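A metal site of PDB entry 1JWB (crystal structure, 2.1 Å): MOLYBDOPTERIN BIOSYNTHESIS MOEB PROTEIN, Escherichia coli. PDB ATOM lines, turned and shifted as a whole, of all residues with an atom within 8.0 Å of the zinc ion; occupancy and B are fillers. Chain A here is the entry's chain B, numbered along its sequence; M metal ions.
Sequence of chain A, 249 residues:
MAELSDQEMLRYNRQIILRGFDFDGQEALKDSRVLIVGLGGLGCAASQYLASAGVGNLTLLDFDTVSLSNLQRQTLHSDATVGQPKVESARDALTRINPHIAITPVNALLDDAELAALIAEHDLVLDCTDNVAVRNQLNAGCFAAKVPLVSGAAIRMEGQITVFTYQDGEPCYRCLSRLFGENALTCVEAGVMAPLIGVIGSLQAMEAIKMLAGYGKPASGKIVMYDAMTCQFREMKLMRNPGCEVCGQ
The side-chain sulfur (SG) of Cys 172 sits close to the backbone NH (N) of Arg 174 (3.4 Å). The side-chain sulfur (SG) of Cys 172 lies close to the side-chain amide oxygen (OD1) of Asn 139 (3.3 Å). SG of Cys 244 sits close to N of Val 246 (3.4 Å). N of Cys 244 sits at hydrogen-bond distance from OD1 of Asn 241 (3.4 Å). O of Cys 247 lies within hydrogen-bond range of NH2 of Arg 240, 2.8 Å away. The side-chain sulfur (SG) of Cys 175 sits close to the backbone NH (N) of Asn 241 (3.3 Å). The guanidinium group (NH1) of Arg 178 sits at hydrogen-bond distance from the backbone carbonyl oxygen (O) of Cys 175 (2.6 Å).
Of the 24 residues printed, 4 come within 4 Å of the zinc ion. The nearest printed residue that does not touch the zinc ion is Arg 174 (4.4 Å).
The zinc ion is bound by SG of Cys 172 (2.2 Å), SG of Cys 244 (2.2 Å), SG of Cys 247 (2.3 Å) and SG of Cys 175 (2.5 Å).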
ATOM      1  N   ASN A 139      12.378  27.537   6.111  1.00  0.00           N
ATOM      2  CA  ASN A 139      11.579  26.637   5.323  1.00  0.00           C
ATOM      3  C   ASN A 139      11.223  25.406   6.112  1.00  0.00           C
ATOM      4  O   ASN A 139      10.112  24.906   6.013  1.00  0.00           O
ATOM      5  CB  ASN A 139      12.310  26.239   4.055  1.00  0.00           C
ATOM      6  CG  ASN A 139      11.652  25.071   3.304  1.00  0.00           C
ATOM      7  OD1 ASN A 139      12.255  23.997   3.143  1.00  0.00           O
ATOM      8  ND2 ASN A 139      10.470  25.297   2.783  1.00  0.00           N
ATOM      9  N   PHE A 143       7.431  24.410   6.886  1.00  0.00           N
ATOM     10  CA  PHE A 143       6.979  23.110   6.427  1.00  0.00           C
ATOM     11  C   PHE A 143       6.357  22.334   7.581  1.00  0.00           C
ATOM     12  O   PHE A 143       5.258  21.817   7.477  1.00  0.00           O
ATOM     13  CB  PHE A 143       8.164  22.302   5.895  1.00  0.00           C
ATOM     14  CG  PHE A 143       7.813  20.898   5.563  1.00  0.00           C
ATOM     15  CD1 PHE A 143       7.046  20.615   4.446  1.00  0.00           C
ATOM     16  CD2 PHE A 143       8.171  19.862   6.394  1.00  0.00           C
ATOM     17  CE1 PHE A 143       6.682  19.317   4.149  1.00  0.00           C
ATOM     18  CE2 PHE A 143       7.803  18.584   6.099  1.00  0.00           C
ATOM     19  CZ  PHE A 143       7.078  18.317   4.993  1.00  0.00           C
ATOM     20  N   PHE A 164       5.788  29.566  -0.727  1.00  0.00           N
ATOM     21  CA  PHE A 164       5.591  28.181  -0.317  1.00  0.00           C
ATOM     22  C   PHE A 164       4.380  28.078   0.609  1.00  0.00           C
ATOM     23  O   PHE A 164       4.354  28.629   1.709  1.00  0.00           O
ATOM     24  CB  PHE A 164       6.828  27.705   0.364  1.00  0.00           C
ATOM     25  CG  PHE A 164       8.031  27.796  -0.487  1.00  0.00           C
ATOM     26  CD1 PHE A 164       8.977  28.784  -0.271  1.00  0.00           C
ATOM     27  CD2 PHE A 164       8.210  26.921  -1.507  1.00  0.00           C
ATOM     28  CE1 PHE A 164      10.087  28.869  -1.041  1.00  0.00           C
ATOM     29  CE2 PHE A 164       9.332  27.003  -2.313  1.00  0.00           C
ATOM     30  CZ  PHE A 164      10.276  27.968  -2.088  1.00  0.00           C
ATOM     31  N   TYR A 166       3.130  25.062   1.298  1.00  0.00           N
ATOM     32  CA  TYR A 166       3.294  23.735   1.867  1.00  0.00           C
ATOM     33  C   TYR A 166       2.107  22.815   1.751  1.00  0.00           C
ATOM     34  O   TYR A 166       1.838  22.079   2.686  1.00  0.00           O
ATOM     35  CB  TYR A 166       3.703  23.824   3.336  1.00  0.00           C
ATOM     36  CG  TYR A 166       4.972  24.572   3.462  1.00  0.00           C
ATOM     37  CD1 TYR A 166       4.970  25.876   3.860  1.00  0.00           C
ATOM     38  CD2 TYR A 166       6.149  23.991   3.111  1.00  0.00           C
ATOM     39  CE1 TYR A 166       6.100  26.566   3.940  1.00  0.00           C
ATOM     40  CE2 TYR A 166       7.291  24.678   3.155  1.00  0.00           C
ATOM     41  CZ  TYR A 166       7.272  25.987   3.570  1.00  0.00           C
ATOM     42  OH  TYR A 166       8.438  26.704   3.651  1.00  0.00           O
ATOM     43  N   GLU A 170       3.390  20.124  -3.221  1.00  0.00           N
ATOM     44  CA  GLU A 170       4.065  21.357  -3.519  1.00  0.00           C
ATOM     45  C   GLU A 170       5.490  21.275  -3.078  1.00  0.00           C
ATOM     46  O   GLU A 170       5.794  20.733  -2.037  1.00  0.00           O
ATOM     47  CB  GLU A 170       3.398  22.504  -2.817  1.00  0.00           C
ATOM     48  CG  GLU A 170       4.222  23.780  -2.820  1.00  0.00           C
ATOM     49  CD  GLU A 170       3.434  24.955  -2.300  1.00  0.00           C
ATOM     50  OE1 GLU A 170       2.237  24.746  -2.039  1.00  0.00           O
ATOM     51  OE2 GLU A 170       4.008  26.064  -2.148  1.00  0.00           O
ATOM     52  N   PRO A 171       6.380  21.856  -3.850  1.00  0.00           N
ATOM     53  CA  PRO A 171       7.791  21.802  -3.476  1.00  0.00           C
ATOM     54  C   PRO A 171       8.009  22.734  -2.319  1.00  0.00           C
ATOM     55  O   PRO A 171       7.223  23.646  -2.098  1.00  0.00           O
ATOM     56  CB  PRO A 171       8.488  22.376  -4.704  1.00  0.00           C
ATOM     57  CG  PRO A 171       7.478  23.349  -5.227  1.00  0.00           C
ATOM     58  CD  PRO A 171       6.144  22.594  -5.103  1.00  0.00           C
ATOM     59  N   CYS A 172       9.080  22.524  -1.616  1.00  0.00           N
ATOM     60  CA  CYS A 172       9.411  23.350  -0.514  1.00  0.00           C
ATOM     61  C   CYS A 172      10.652  24.157  -0.962  1.00  0.00           C
ATOM     62  O   CYS A 172      11.102  24.029  -2.087  1.00  0.00           O
ATOM     63  CB  CYS A 172       9.650  22.508   0.749  1.00  0.00           C
ATOM     64  SG  CYS A 172      11.238  21.759   0.898  1.00  0.00           S
ATOM     65  N   TYR A 173      11.221  24.963  -0.081  1.00  0.00           N
ATOM     66  CA  TYR A 173      12.374  25.767  -0.470  1.00  0.00           C
ATOM     67  C   TYR A 173      13.667  24.971  -0.688  1.00  0.00           C
ATOM     68  O   TYR A 173      14.522  25.338  -1.512  1.00  0.00           O
ATOM     69  CB  TYR A 173      12.640  26.864   0.530  1.00  0.00           C
ATOM     70  CG  TYR A 173      13.836  27.674   0.149  1.00  0.00           C
ATOM     71  CD1 TYR A 173      13.785  28.568  -0.904  1.00  0.00           C
ATOM     72  CD2 TYR A 173      15.028  27.555   0.856  1.00  0.00           C
ATOM     73  CE1 TYR A 173      14.862  29.337  -1.211  1.00  0.00           C
ATOM     74  CE2 TYR A 173      16.106  28.286   0.525  1.00  0.00           C
ATOM     75  CZ  TYR A 173      16.016  29.191  -0.505  1.00  0.00           C
ATOM     76  OH  TYR A 173      17.114  29.913  -0.885  1.00  0.00           O
ATOM     77  N   ARG A 174      13.822  23.883   0.063  1.00  0.00           N
ATOM     78  CA  ARG A 174      14.946  22.972  -0.125  1.00  0.00           C
ATOM     79  C   ARG A 174      14.854  22.275  -1.486  1.00  0.00           C
ATOM     80  O   ARG A 174      15.858  21.970  -2.094  1.00  0.00           O
ATOM     81  CB  ARG A 174      14.973  21.968   1.020  1.00  0.00           C
ATOM     82  CG  ARG A 174      16.205  21.113   1.067  1.00  0.00           C
ATOM     83  CD  ARG A 174      17.470  21.883   1.312  1.00  0.00           C
ATOM     84  NE  ARG A 174      18.601  20.999   1.093  1.00  0.00           N
ATOM     85  CZ  ARG A 174      19.821  21.365   0.694  1.00  0.00           C
ATOM     86  NH1 ARG A 174      20.132  22.650   0.460  1.00  0.00           N
ATOM     87  NH2 ARG A 174      20.749  20.426   0.542  1.00  0.00           N
ATOM     88  N   CYS A 175      13.631  22.076  -1.941  1.00  0.00           N
ATOM     89  CA  CYS A 175      13.471  21.538  -3.277  1.00  0.00           C
ATOM     90  C   CYS A 175      14.286  22.387  -4.221  1.00  0.00           C
ATOM     91  O   CYS A 175      14.802  21.895  -5.233  1.00  0.00           O
ATOM     92  CB  CYS A 175      12.021  21.557  -3.737  1.00  0.00           C
ATOM     93  SG  CYS A 175      11.039  20.227  -3.062  1.00  0.00           S
ATOM     94  N   LEU A 176      14.324  23.681  -3.919  1.00  0.00           N
ATOM     95  CA  LEU A 176      15.085  24.661  -4.697  1.00  0.00           C
ATOM     96  C   LEU A 176      16.507  24.771  -4.238  1.00  0.00           C
ATOM     97  O   LEU A 176      17.422  24.767  -5.052  1.00  0.00           O
ATOM     98  CB  LEU A 176      14.420  26.046  -4.635  1.00  0.00           C
ATOM     99  CG  LEU A 176      15.231  27.270  -5.132  1.00  0.00           C
ATOM    100  CD1 LEU A 176      15.770  27.086  -6.542  1.00  0.00           C
ATOM    101  CD2 LEU A 176      14.424  28.579  -5.065  1.00  0.00           C
ATOM    102  N   SER A 177      16.733  24.895  -2.940  1.00  0.00           N
ATOM    103  CA  SER A 177      18.090  25.200  -2.495  1.00  0.00           C
ATOM    104  C   SER A 177      19.029  24.045  -2.692  1.00  0.00           C
ATOM    105  O   SER A 177      20.264  24.245  -2.712  1.00  0.00           O
ATOM    106  CB  SER A 177      18.143  25.735  -1.053  1.00  0.00           C
ATOM    107  OG  SER A 177      17.861  24.784  -0.061  1.00  0.00           O
ATOM    108  N   ARG A 178      18.470  22.834  -2.827  1.00  0.00           N
ATOM    109  CA  ARG A 178      19.320  21.672  -3.081  1.00  0.00           C
ATOM    110  C   ARG A 178      19.924  21.786  -4.493  1.00  0.00           C
ATOM    111  O   ARG A 178      20.884  21.090  -4.799  1.00  0.00           O
ATOM    112  CB  ARG A 178      18.626  20.282  -2.783  1.00  0.00           C
ATOM    113  CG  ARG A 178      17.372  19.777  -3.573  1.00  0.00           C
ATOM    114  CD  ARG A 178      17.236  20.150  -5.081  1.00  0.00           C
ATOM    115  NE  ARG A 178      16.757  19.039  -5.944  1.00  0.00           N
ATOM    116  CZ  ARG A 178      15.867  19.149  -6.943  1.00  0.00           C
ATOM    117  NH1 ARG A 178      15.289  20.312  -7.223  1.00  0.00           N
ATOM    118  NH2 ARG A 178      15.551  18.088  -7.683  1.00  0.00           N
ATOM    119  N   LEU A 238       8.561  25.261 -10.380  1.00  0.00           N
ATOM    120  CA  LEU A 238       9.343  24.549  -9.385  1.00  0.00           C
ATOM    121  C   LEU A 238       8.607  23.278  -9.031  1.00  0.00           C
ATOM    122  O   LEU A 238       7.437  23.297  -8.620  1.00  0.00           O
ATOM    123  CB  LEU A 238       9.558  25.440  -8.158  1.00  0.00           C
ATOM    124  CG  LEU A 238      10.265  24.906  -6.923  1.00  0.00           C
ATOM    125  CD1 LEU A 238      11.698  24.488  -7.115  1.00  0.00           C
ATOM    126  CD2 LEU A 238      10.229  25.954  -5.867  1.00  0.00           C
ATOM    127  N   MET A 239       9.277  22.153  -9.258  1.00  0.00           N
ATOM    128  CA  MET A 239       8.735  20.854  -8.914  1.00  0.00           C
ATOM    129  C   MET A 239       9.311  20.301  -7.630  1.00  0.00           C
ATOM    130  O   MET A 239      10.461  20.545  -7.285  1.00  0.00           O
ATOM    131  CB  MET A 239       9.100  19.866 -10.001  1.00  0.00           C
ATOM    132  CG  MET A 239       8.711  20.361 -11.378  1.00  0.00           C
ATOM    133  SD  MET A 239       6.987  20.173 -11.648  1.00  0.00           S
ATOM    134  CE  MET A 239       6.891  18.349 -11.615  1.00  0.00           C
ATOM    135  N   ARG A 240       8.518  19.475  -6.964  1.00  0.00           N
ATOM    136  CA  ARG A 240       8.947  18.835  -5.739  1.00  0.00           C
ATOM    137  C   ARG A 240      10.018  17.810  -6.048  1.00  0.00           C
ATOM    138  O   ARG A 240       9.863  17.039  -6.977  1.00  0.00           O
ATOM    139  CB  ARG A 240       7.759  18.104  -5.122  1.00  0.00           C
ATOM    140  CG  ARG A 240       7.984  17.548  -3.732  1.00  0.00           C
ATOM    141  CD  ARG A 240       6.712  17.672  -2.893  1.00  0.00           C
ATOM    142  NE  ARG A 240       6.827  17.241  -1.500  1.00  0.00           N
ATOM    143  CZ  ARG A 240       5.989  17.612  -0.516  1.00  0.00           C
ATOM    144  NH1 ARG A 240       4.984  18.451  -0.749  1.00  0.00           N
ATOM    145  NH2 ARG A 240       6.191  17.148   0.711  1.00  0.00           N
ATOM    146  N   ASN A 241      11.112  17.820  -5.288  1.00  0.00           N
ATOM    147  CA  ASN A 241      12.148  16.809  -5.448  1.00  0.00           C
ATOM    148  C   ASN A 241      11.885  15.606  -4.538  1.00  0.00           C
ATOM    149  O   ASN A 241      11.969  15.697  -3.317  1.00  0.00           O
ATOM    150  CB  ASN A 241      13.538  17.409  -5.226  1.00  0.00           C
ATOM    151  CG  ASN A 241      14.627  16.366  -5.111  1.00  0.00           C
ATOM    152  OD1 ASN A 241      15.524  16.507  -4.279  1.00  0.00           O
ATOM    153  ND2 ASN A 241      14.570  15.329  -5.928  1.00  0.00           N
ATOM    154  N   PRO A 242      11.569  14.488  -5.169  1.00  0.00           N
ATOM    155  CA  PRO A 242      11.280  13.216  -4.510  1.00  0.00           C
ATOM    156  C   PRO A 242      12.025  12.987  -3.216  1.00  0.00           C
ATOM    157  O   PRO A 242      11.439  12.569  -2.227  1.00  0.00           O
ATOM    158  CB  PRO A 242      11.818  12.206  -5.526  1.00  0.00           C
ATOM    159  CG  PRO A 242      12.238  13.031  -6.761  1.00  0.00           C
ATOM    160  CD  PRO A 242      11.503  14.334  -6.633  1.00  0.00           C
ATOM    161  N   GLY A 243      13.334  13.213  -3.257  1.00  0.00           N
ATOM    162  CA  GLY A 243      14.177  13.008  -2.084  1.00  0.00           C
ATOM    163  C   GLY A 243      14.616  14.304  -1.411  1.00  0.00           C
ATOM    164  O   GLY A 243      15.675  14.349  -0.785  1.00  0.00           O
ATOM    165  N   CYS A 244      13.805  15.356  -1.547  1.00  0.00           N
ATOM    166  CA  CYS A 244      14.083  16.592  -0.851  1.00  0.00           C
ATOM    167  C   CYS A 244      14.193  16.106   0.559  1.00  0.00           C
ATOM    168  O   CYS A 244      13.321  15.388   1.028  1.00  0.00           O
ATOM    169  CB  CYS A 244      12.904  17.577  -0.954  1.00  0.00           C
ATOM    170  SG  CYS A 244      12.979  19.001   0.177  1.00  0.00           S
ATOM    171  N   GLU A 245      15.262  16.534   1.240  1.00  0.00           N
ATOM    172  CA  GLU A 245      15.510  16.195   2.644  1.00  0.00           C
ATOM    173  C   GLU A 245      14.343  16.647   3.536  1.00  0.00           C
ATOM    174  O   GLU A 245      13.916  15.937   4.458  1.00  0.00           O
ATOM    175  CB  GLU A 245      16.817  16.877   3.120  1.00  0.00           C
ATOM    176  CG  GLU A 245      18.071  16.586   2.280  1.00  0.00           C
ATOM    177  CD  GLU A 245      18.271  17.516   1.059  1.00  0.00           C
ATOM    178  OE1 GLU A 245      17.292  17.877   0.342  1.00  0.00           O
ATOM    179  OE2 GLU A 245      19.445  17.857   0.777  1.00  0.00           O
ATOM    180  N   VAL A 246      13.827  17.838   3.272  1.00  0.00           N
ATOM    181  CA  VAL A 246      12.734  18.335   4.082  1.00  0.00           C
ATOM    182  C   VAL A 246      11.378  17.782   3.644  1.00  0.00           C
ATOM    183  O   VAL A 246      10.634  17.258   4.481  1.00  0.00           O
ATOM    184  CB  VAL A 246      12.653  19.866   4.033  1.00  0.00           C
ATOM    185  CG1 VAL A 246      11.291  20.334   4.587  1.00  0.00           C
ATOM    186  CG2 VAL A 246      13.835  20.484   4.803  1.00  0.00           C
ATOM    187  N   CYS A 247      11.016  17.939   2.373  1.00  0.00           N
ATOM    188  CA  CYS A 247       9.663  17.534   1.980  1.00  0.00           C
ATOM    189  C   CYS A 247       9.627  16.202   1.244  1.00  0.00           C
ATOM    190  O   CYS A 247       8.570  15.754   0.851  1.00  0.00           O
ATOM    191  CB  CYS A 247       8.932  18.662   1.208  1.00  0.00           C
ATOM    192  SG  CYS A 247       9.275  18.826  -0.560  1.00  0.00           S
ATOM    193  N   GLY A 248      10.771  15.555   1.096  1.00  0.00           N
ATOM    194  CA  GLY A 248      10.829  14.303   0.339  1.00  0.00           C
ATOM    195  C   GLY A 248      10.273  13.097   1.075  1.00  0.00           C
ATOM    196  O   GLY A 248       9.062  13.005   1.298  1.00  0.00           O
HETATM  197 ZN    ZN M   1      11.156  20.074  -0.561  1.00  0.00          ZN
